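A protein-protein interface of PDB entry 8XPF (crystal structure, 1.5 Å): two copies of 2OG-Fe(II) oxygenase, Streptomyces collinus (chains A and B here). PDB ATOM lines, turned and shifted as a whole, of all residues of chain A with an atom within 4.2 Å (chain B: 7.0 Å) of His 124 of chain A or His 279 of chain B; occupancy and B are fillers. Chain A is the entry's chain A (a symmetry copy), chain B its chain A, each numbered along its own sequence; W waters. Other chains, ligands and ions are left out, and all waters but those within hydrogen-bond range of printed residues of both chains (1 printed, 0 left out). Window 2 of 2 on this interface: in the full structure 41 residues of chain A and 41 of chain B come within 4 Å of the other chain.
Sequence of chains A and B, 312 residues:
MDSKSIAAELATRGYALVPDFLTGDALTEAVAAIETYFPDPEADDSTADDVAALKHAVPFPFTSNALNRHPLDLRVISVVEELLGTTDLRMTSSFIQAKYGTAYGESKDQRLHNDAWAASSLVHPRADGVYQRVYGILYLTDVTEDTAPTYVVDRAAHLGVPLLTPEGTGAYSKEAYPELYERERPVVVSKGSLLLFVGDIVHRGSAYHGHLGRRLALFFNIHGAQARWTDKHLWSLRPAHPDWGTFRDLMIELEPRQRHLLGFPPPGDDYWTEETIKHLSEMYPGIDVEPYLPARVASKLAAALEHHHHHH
Among the printed residues, merely in contact across the chains: Trp 117 of chain A with Met 283 of chain B (3.8 Å), Val 123 of chain A with Tyr 271 of chain B (3.4 Å), His 124 of chain A with His 279 of chain B (3.6 Å), His 124 of chain A with Met 283 of chain B (3.8 Å), Arg 126 of chain A with Thr 273 of chain B (3.6 Å) and Arg 126 of chain A with Thr 276 of chain B (3.6 Å).
Of the printed residues of chain B, Val 123 of chain A touches Tyr 271.
His 124 of chain A touches just these residues of chain B: Tyr 271 (2.6 Å), His 279 (3.6 Å) and Met 283 (3.8 Å).
Of the printed residues of chain B, Arg 126 of chain A touches Tyr 271, Thr 273 and Thr 276.
Printed residues of chain A within 4 Å of Thr 273 of chain B: Arg 126 (3.6 Å).
Ile 277 of chain B touches none of the printed residues of chain A.
Of the printed residues of chain A, His 279 of chain B touches His 124 (3.6 Å).
Of the printed residues of chain A, Met 283 of chain B touches Trp 117 and His 124.
The nearest printed residue of chain A that does not touch Tyr 271 of chain B is Pro 125 of chain A (4.7 Å).
No position is printed for both chains.
Of the 13 printed residues of chain B, 5 touch a printed residue of chain A.
Hydrophobic or aromatic side chains of chain B that line the printed part of chain A: Tyr 271, His 279 and Met 283.
Of the 6 printed residues of chain A, 4 touch a printed residue of chain B.
Among the printed residues, 8 pairs touch across the chains.
Among the printed residues, no Asp or Glu carboxylate lies within 4 Å of a Lys or Arg side-chain nitrogen of the other chain.
Water W1 bridges N of His 124 of chain A (2.9 Å) and SD of Met 283 of chain B (3.3 Å).
O of Tyr 271 of chain B sits at hydrogen-bond distance from OG1 of Thr 276 of chain B (2.8 Å).
OG1 of Thr 273 of chain B sits close to N of Glu 275 of chain B (3.2 Å).
The backbone NH of Thr 273 of chain B sits at hydrogen-bond distance from the side-chain hydroxyl of Thr 276 of chain B (2.8 Å).
NE2 of His 279 of chain B is in hydrogen-bond range of OE2 of Glu 275 of chain B, 3.4 Å away.
OE1 of Glu 282 of chain B is in hydrogen-bond range of ND1 of His 279 of chain B, 2.8 Å away.
The indole nitrogen of Trp 117 of chain A lies within hydrogen-bond range of the backbone carbonyl oxygen of Leu 163 of chain A, 2.9 Å away.
The backbone carbonyl oxygen (O) of His 124 of chain A lies within hydrogen-bond range of the side-chain hydroxyl (OH) of Tyr 271 of chain B (2.6 Å).
O of Tyr 271 of chain B sits at hydrogen-bond distance from NH1 of Arg 126 of chain A, at 3.0 Å.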
ATOM      1  N   TRP A 117      30.971  38.948 -20.577  1.00  0.00           N
ATOM      2  CA  TRP A 117      31.680  38.383 -19.433  1.00  0.00           C
ATOM      3  C   TRP A 117      31.753  39.350 -18.256  1.00  0.00           C
ATOM      4  O   TRP A 117      31.901  40.563 -18.423  1.00  0.00           O
ATOM      5  CB  TRP A 117      33.117  38.056 -19.846  1.00  0.00           C
ATOM      6  CG  TRP A 117      33.220  36.897 -20.761  1.00  0.00           C
ATOM      7  CD1 TRP A 117      33.041  36.893 -22.127  1.00  0.00           C
ATOM      8  CD2 TRP A 117      33.493  35.552 -20.384  1.00  0.00           C
ATOM      9  NE1 TRP A 117      33.198  35.619 -22.606  1.00  0.00           N
ATOM     10  CE2 TRP A 117      33.478  34.775 -21.563  1.00  0.00           C
ATOM     11  CE3 TRP A 117      33.746  34.919 -19.153  1.00  0.00           C
ATOM     12  CZ2 TRP A 117      33.714  33.404 -21.549  1.00  0.00           C
ATOM     13  CZ3 TRP A 117      33.982  33.557 -19.146  1.00  0.00           C
ATOM     14  CH2 TRP A 117      33.961  32.815 -20.334  1.00  0.00           C
ATOM     15  N   VAL A 123      32.756  32.484 -14.155  1.00  0.00           N
ATOM     16  CA  VAL A 123      32.021  31.441 -14.870  1.00  0.00           C
ATOM     17  C   VAL A 123      31.619  31.960 -16.243  1.00  0.00           C
ATOM     18  O   VAL A 123      31.549  33.165 -16.492  1.00  0.00           O
ATOM     19  CB  VAL A 123      30.775  30.918 -14.113  1.00  0.00           C
ATOM     20  CG1 VAL A 123      31.171  30.276 -12.777  1.00  0.00           C
ATOM     21  CG2 VAL A 123      29.750  32.044 -13.898  1.00  0.00           C
ATOM     22  N   HIS A 124      31.322  31.016 -17.124  1.00  0.00           N
ATOM     23  CA  HIS A 124      30.972  31.346 -18.491  1.00  0.00           C
ATOM     24  C   HIS A 124      29.644  32.104 -18.514  1.00  0.00           C
ATOM     25  O   HIS A 124      28.728  31.783 -17.747  1.00  0.00           O
ATOM     26  CB  HIS A 124      30.827  30.034 -19.263  1.00  0.00           C
ATOM     27  CG  HIS A 124      30.753  30.185 -20.749  1.00  0.00           C
ATOM     28  ND1 HIS A 124      29.627  30.649 -21.391  1.00  0.00           N
ATOM     29  CD2 HIS A 124      31.650  29.893 -21.723  1.00  0.00           C
ATOM     30  CE1 HIS A 124      29.833  30.642 -22.698  1.00  0.00           C
ATOM     31  NE2 HIS A 124      31.050  30.184 -22.925  1.00  0.00           N
ATOM     32  N   PRO A 125      29.490  33.075 -19.402  1.00  0.00           N
ATOM     33  CA  PRO A 125      28.227  33.817 -19.474  1.00  0.00           C
ATOM     34  C   PRO A 125      27.067  32.960 -19.963  1.00  0.00           C
ATOM     35  O   PRO A 125      27.229  31.927 -20.624  1.00  0.00           O
ATOM     36  CB  PRO A 125      28.519  34.934 -20.484  1.00  0.00           C
ATOM     37  CG  PRO A 125      29.998  34.985 -20.634  1.00  0.00           C
ATOM     38  CD  PRO A 125      30.519  33.613 -20.305  1.00  0.00           C
ATOM     39  N   ARG A 126      25.868  33.445 -19.656  1.00  0.00           N
ATOM     40  CA  ARG A 126      24.635  33.045 -20.323  1.00  0.00           C
ATOM     41  C   ARG A 126      24.035  34.270 -20.997  1.00  0.00           C
ATOM     42  O   ARG A 126      24.102  35.378 -20.466  1.00  0.00           O
ATOM     43  CB  ARG A 126      23.636  32.455 -19.335  1.00  0.00           C
ATOM     44  CG  ARG A 126      23.936  31.018 -18.995  1.00  0.00           C
ATOM     45  CD  ARG A 126      23.064  30.512 -17.859  1.00  0.00           C
ATOM     46  NE  ARG A 126      21.636  30.536 -18.168  1.00  0.00           N
ATOM     47  CZ  ARG A 126      20.703  30.005 -17.388  1.00  0.00           C
ATOM     48  NH1 ARG A 126      21.017  29.358 -16.274  1.00  0.00           N
ATOM     49  NH2 ARG A 126      19.422  30.132 -17.726  1.00  0.00           N
ATOM     50  N   LEU A 163      31.017  32.636 -27.175  1.00  0.00           N
ATOM     51  CA  LEU A 163      31.343  33.737 -26.280  1.00  0.00           C
ATOM     52  C   LEU A 163      32.780  33.658 -25.769  1.00  0.00           C
ATOM     53  O   LEU A 163      33.349  34.695 -25.399  1.00  0.00           O
ATOM     54  CB  LEU A 163      30.360  33.780 -25.113  1.00  0.00           C
ATOM     55  CG  LEU A 163      28.925  34.132 -25.509  1.00  0.00           C
ATOM     56  CD1 LEU A 163      28.037  34.139 -24.287  1.00  0.00           C
ATOM     57  CD2 LEU A 163      28.870  35.479 -26.220  1.00  0.00           C
ATOM     58  N   TYR B 271      21.581  29.346 -12.146  1.00  0.00           N
ATOM     59  CA  TYR B 271      22.604  29.420 -13.183  1.00  0.00           C
ATOM     60  C   TYR B 271      22.944  28.042 -13.744  1.00  0.00           C
ATOM     61  O   TYR B 271      23.265  27.921 -14.931  1.00  0.00           O
ATOM     62  CB  TYR B 271      23.855  30.130 -12.645  1.00  0.00           C
ATOM     63  CG  TYR B 271      25.049  30.050 -13.572  1.00  0.00           C
ATOM     64  CD1 TYR B 271      25.210  30.974 -14.601  1.00  0.00           C
ATOM     65  CD2 TYR B 271      26.018  29.059 -13.414  1.00  0.00           C
ATOM     66  CE1 TYR B 271      26.299  30.904 -15.461  1.00  0.00           C
ATOM     67  CE2 TYR B 271      27.114  28.980 -14.271  1.00  0.00           C
ATOM     68  CZ  TYR B 271      27.253  29.903 -15.284  1.00  0.00           C
ATOM     69  OH  TYR B 271      28.326  29.811 -16.155  1.00  0.00           O
ATOM     70  N   THR B 273      22.844  24.624 -15.427  1.00  0.00           N
ATOM     71  CA  THR B 273      22.118  23.841 -16.416  1.00  0.00           C
ATOM     72  C   THR B 273      23.106  22.870 -17.042  1.00  0.00           C
ATOM     73  O   THR B 273      24.310  22.934 -16.792  1.00  0.00           O
ATOM     74  CB  THR B 273      21.569  24.730 -17.536  1.00  0.00           C
ATOM     75  OG1 THR B 273      22.666  25.306 -18.257  1.00  0.00           O
ATOM     76  CG2 THR B 273      20.690  25.840 -16.972  1.00  0.00           C
ATOM     77  N   GLU B 274      22.602  21.972 -17.890  1.00  0.00           N
ATOM     78  CA  GLU B 274      23.517  21.091 -18.609  1.00  0.00           C
ATOM     79  C   GLU B 274      24.580  21.891 -19.350  1.00  0.00           C
ATOM     80  O   GLU B 274      25.765  21.533 -19.339  1.00  0.00           O
ATOM     81  CB  GLU B 274      22.748  20.200 -19.581  1.00  0.00           C
ATOM     82  CG  GLU B 274      22.014  19.053 -18.927  1.00  0.00           C
ATOM     83  CD  GLU B 274      21.550  18.023 -19.938  1.00  0.00           C
ATOM     84  OE1 GLU B 274      21.715  18.266 -21.157  1.00  0.00           O
ATOM     85  OE2 GLU B 274      21.025  16.970 -19.517  1.00  0.00           O
ATOM     86  N   GLU B 275      24.180  23.003 -19.974  1.00  0.00           N
ATOM     87  CA  GLU B 275      25.141  23.793 -20.735  1.00  0.00           C
ATOM     88  C   GLU B 275      26.169  24.475 -19.838  1.00  0.00           C
ATOM     89  O   GLU B 275      27.350  24.536 -20.193  1.00  0.00           O
ATOM     90  CB  GLU B 275      24.444  24.830 -21.610  1.00  0.00           C
ATOM     91  CG  GLU B 275      25.449  25.683 -22.381  1.00  0.00           C
ATOM     92  CD  GLU B 275      24.848  26.417 -23.567  1.00  0.00           C
ATOM     93  OE1 GLU B 275      23.627  26.702 -23.548  1.00  0.00           O
ATOM     94  OE2 GLU B 275      25.608  26.702 -24.522  1.00  0.00           O
ATOM     95  N   THR B 276      25.748  25.049 -18.705  1.00  0.00           N
ATOM     96  CA  THR B 276      26.752  25.720 -17.880  1.00  0.00           C
ATOM     97  C   THR B 276      27.618  24.741 -17.102  1.00  0.00           C
ATOM     98  O   THR B 276      28.754  25.073 -16.766  1.00  0.00           O
ATOM     99  CB  THR B 276      26.147  26.763 -16.936  1.00  0.00           C
ATOM    100  OG1 THR B 276      25.118  26.176 -16.137  1.00  0.00           O
ATOM    101  CG2 THR B 276      25.598  27.947 -17.720  1.00  0.00           C
ATOM    102  N   ILE B 277      27.122  23.536 -16.809  1.00  0.00           N
ATOM    103  CA  ILE B 277      28.016  22.532 -16.243  1.00  0.00           C
ATOM    104  C   ILE B 277      29.096  22.174 -17.259  1.00  0.00           C
ATOM    105  O   ILE B 277      30.291  22.107 -16.929  1.00  0.00           O
ATOM    106  CB  ILE B 277      27.221  21.297 -15.778  1.00  0.00           C
ATOM    107  CG1 ILE B 277      26.323  21.650 -14.584  1.00  0.00           C
ATOM    108  CG2 ILE B 277      28.177  20.157 -15.426  1.00  0.00           C
ATOM    109  CD1 ILE B 277      27.072  21.834 -13.273  1.00  0.00           C
ATOM    110  N   LYS B 278      28.697  21.995 -18.523  1.00  0.00           N
ATOM    111  CA  LYS B 278      29.663  21.721 -19.582  1.00  0.00           C
ATOM    112  C   LYS B 278      30.689  22.842 -19.687  1.00  0.00           C
ATOM    113  O   LYS B 278      31.896  22.592 -19.770  1.00  0.00           O
ATOM    114  CB  LYS B 278      28.953  21.533 -20.925  1.00  0.00           C
ATOM    115  CG  LYS B 278      29.927  21.379 -22.094  1.00  0.00           C
ATOM    116  CD  LYS B 278      29.235  21.349 -23.454  1.00  0.00           C
ATOM    117  CE  LYS B 278      29.609  22.580 -24.285  1.00  0.00           C
ATOM    118  NZ  LYS B 278      29.239  22.408 -25.726  1.00  0.00           N
ATOM    119  N   HIS B 279      30.228  24.093 -19.705  1.00  0.00           N
ATOM    120  CA  HIS B 279      31.183  25.188 -19.824  1.00  0.00           C
ATOM    121  C   HIS B 279      32.098  25.269 -18.610  1.00  0.00           C
ATOM    122  O   HIS B 279      33.259  25.679 -18.728  1.00  0.00           O
ATOM    123  CB  HIS B 279      30.456  26.519 -20.054  1.00  0.00           C
ATOM    124  CG  HIS B 279      29.929  26.691 -21.444  1.00  0.00           C
ATOM    125  ND1 HIS B 279      30.647  26.338 -22.566  1.00  0.00           N
ATOM    126  CD2 HIS B 279      28.751  27.184 -21.893  1.00  0.00           C
ATOM    127  CE1 HIS B 279      29.933  26.603 -23.646  1.00  0.00           C
ATOM    128  NE2 HIS B 279      28.778  27.120 -23.265  1.00  0.00           N
ATOM    129  N   LEU B 280      31.603  24.898 -17.430  1.00  0.00           N
ATOM    130  CA  LEU B 280      32.467  24.919 -16.260  1.00  0.00           C
ATOM    131  C   LEU B 280      33.595  23.905 -16.408  1.00  0.00           C
ATOM    132  O   LEU B 280      34.761  24.211 -16.132  1.00  0.00           O
ATOM    133  CB  LEU B 280      31.646  24.648 -15.004  1.00  0.00           C
ATOM    134  CG  LEU B 280      32.390  24.822 -13.682  1.00  0.00           C
ATOM    135  CD1 LEU B 280      32.617  26.298 -13.383  1.00  0.00           C
ATOM    136  CD2 LEU B 280      31.605  24.152 -12.567  1.00  0.00           C
ATOM    137  N   SER B 281      33.264  22.687 -16.849  1.00  0.00           N
ATOM    138  CA  SER B 281      34.287  21.667 -17.059  1.00  0.00           C
ATOM    139  C   SER B 281      35.290  22.085 -18.120  1.00  0.00           C
ATOM    140  O   SER B 281      36.471  21.724 -18.030  1.00  0.00           O
ATOM    141  CB  SER B 281      33.642  20.330 -17.422  1.00  0.00           C
ATOM    142  OG  SER B 281      32.885  19.857 -16.324  1.00  0.00           O
ATOM    143  N   GLU B 282      34.842  22.819 -19.141  1.00  0.00           N
ATOM    144  CA  GLU B 282      35.750  23.263 -20.195  1.00  0.00           C
ATOM    145  C   GLU B 282      36.750  24.281 -19.666  1.00  0.00           C
ATOM    146  O   GLU B 282      37.948  24.206 -19.972  1.00  0.00           O
ATOM    147  CB  GLU B 282      34.958  23.856 -21.365  1.00  0.00           C
ATOM    148  CG  GLU B 282      34.148  22.883 -22.187  1.00  0.00           C
ATOM    149  CD  GLU B 282      33.250  23.594 -23.199  1.00  0.00           C
ATOM    150  OE1 GLU B 282      32.968  24.805 -22.997  1.00  0.00           O
ATOM    151  OE2 GLU B 282      32.813  22.943 -24.169  1.00  0.00           O
ATOM    152  N   MET B 283      36.278  25.241 -18.869  1.00  0.00           N
ATOM    153  CA  MET B 283      37.151  26.288 -18.360  1.00  0.00           C
ATOM    154  C   MET B 283      38.055  25.798 -17.240  1.00  0.00           C
ATOM    155  O   MET B 283      39.151  26.336 -17.059  1.00  0.00           O
ATOM    156  CB  MET B 283      36.317  27.469 -17.865  1.00  0.00           C
ATOM    157  CG  MET B 283      35.768  28.292 -19.018  1.00  0.00           C
ATOM    158  SD  MET B 283      34.625  29.549 -18.408  1.00  0.00           S
ATOM    159  CE  MET B 283      35.636  30.482 -17.256  1.00  0.00           C
ATOM    160  N   TYR B 284      37.615  24.806 -16.473  1.00  0.00           N
ATOM    161  CA  TYR B 284      38.354  24.335 -15.304  1.00  0.00           C
ATOM    162  C   TYR B 284      38.490  22.821 -15.396  1.00  0.00           C
ATOM    163  O   TYR B 284      37.868  22.088 -14.618  1.00  0.00           O
ATOM    164  CB  TYR B 284      37.610  24.727 -14.029  1.00  0.00           C
ATOM    165  CG  TYR B 284      37.406  26.224 -13.825  1.00  0.00           C
ATOM    166  CD1 TYR B 284      38.465  27.036 -13.473  1.00  0.00           C
ATOM    167  CD2 TYR B 284      36.152  26.801 -13.955  1.00  0.00           C
ATOM    168  CE1 TYR B 284      38.286  28.391 -13.256  1.00  0.00           C
ATOM    169  CE2 TYR B 284      35.951  28.169 -13.741  1.00  0.00           C
ATOM    170  CZ  TYR B 284      37.038  28.951 -13.381  1.00  0.00           C
ATOM    171  OH  TYR B 284      36.898  30.307 -13.163  1.00  0.00           O
HETATM  172  O   HOH W   1      32.298  28.348 -16.440  1.00  0.00           O
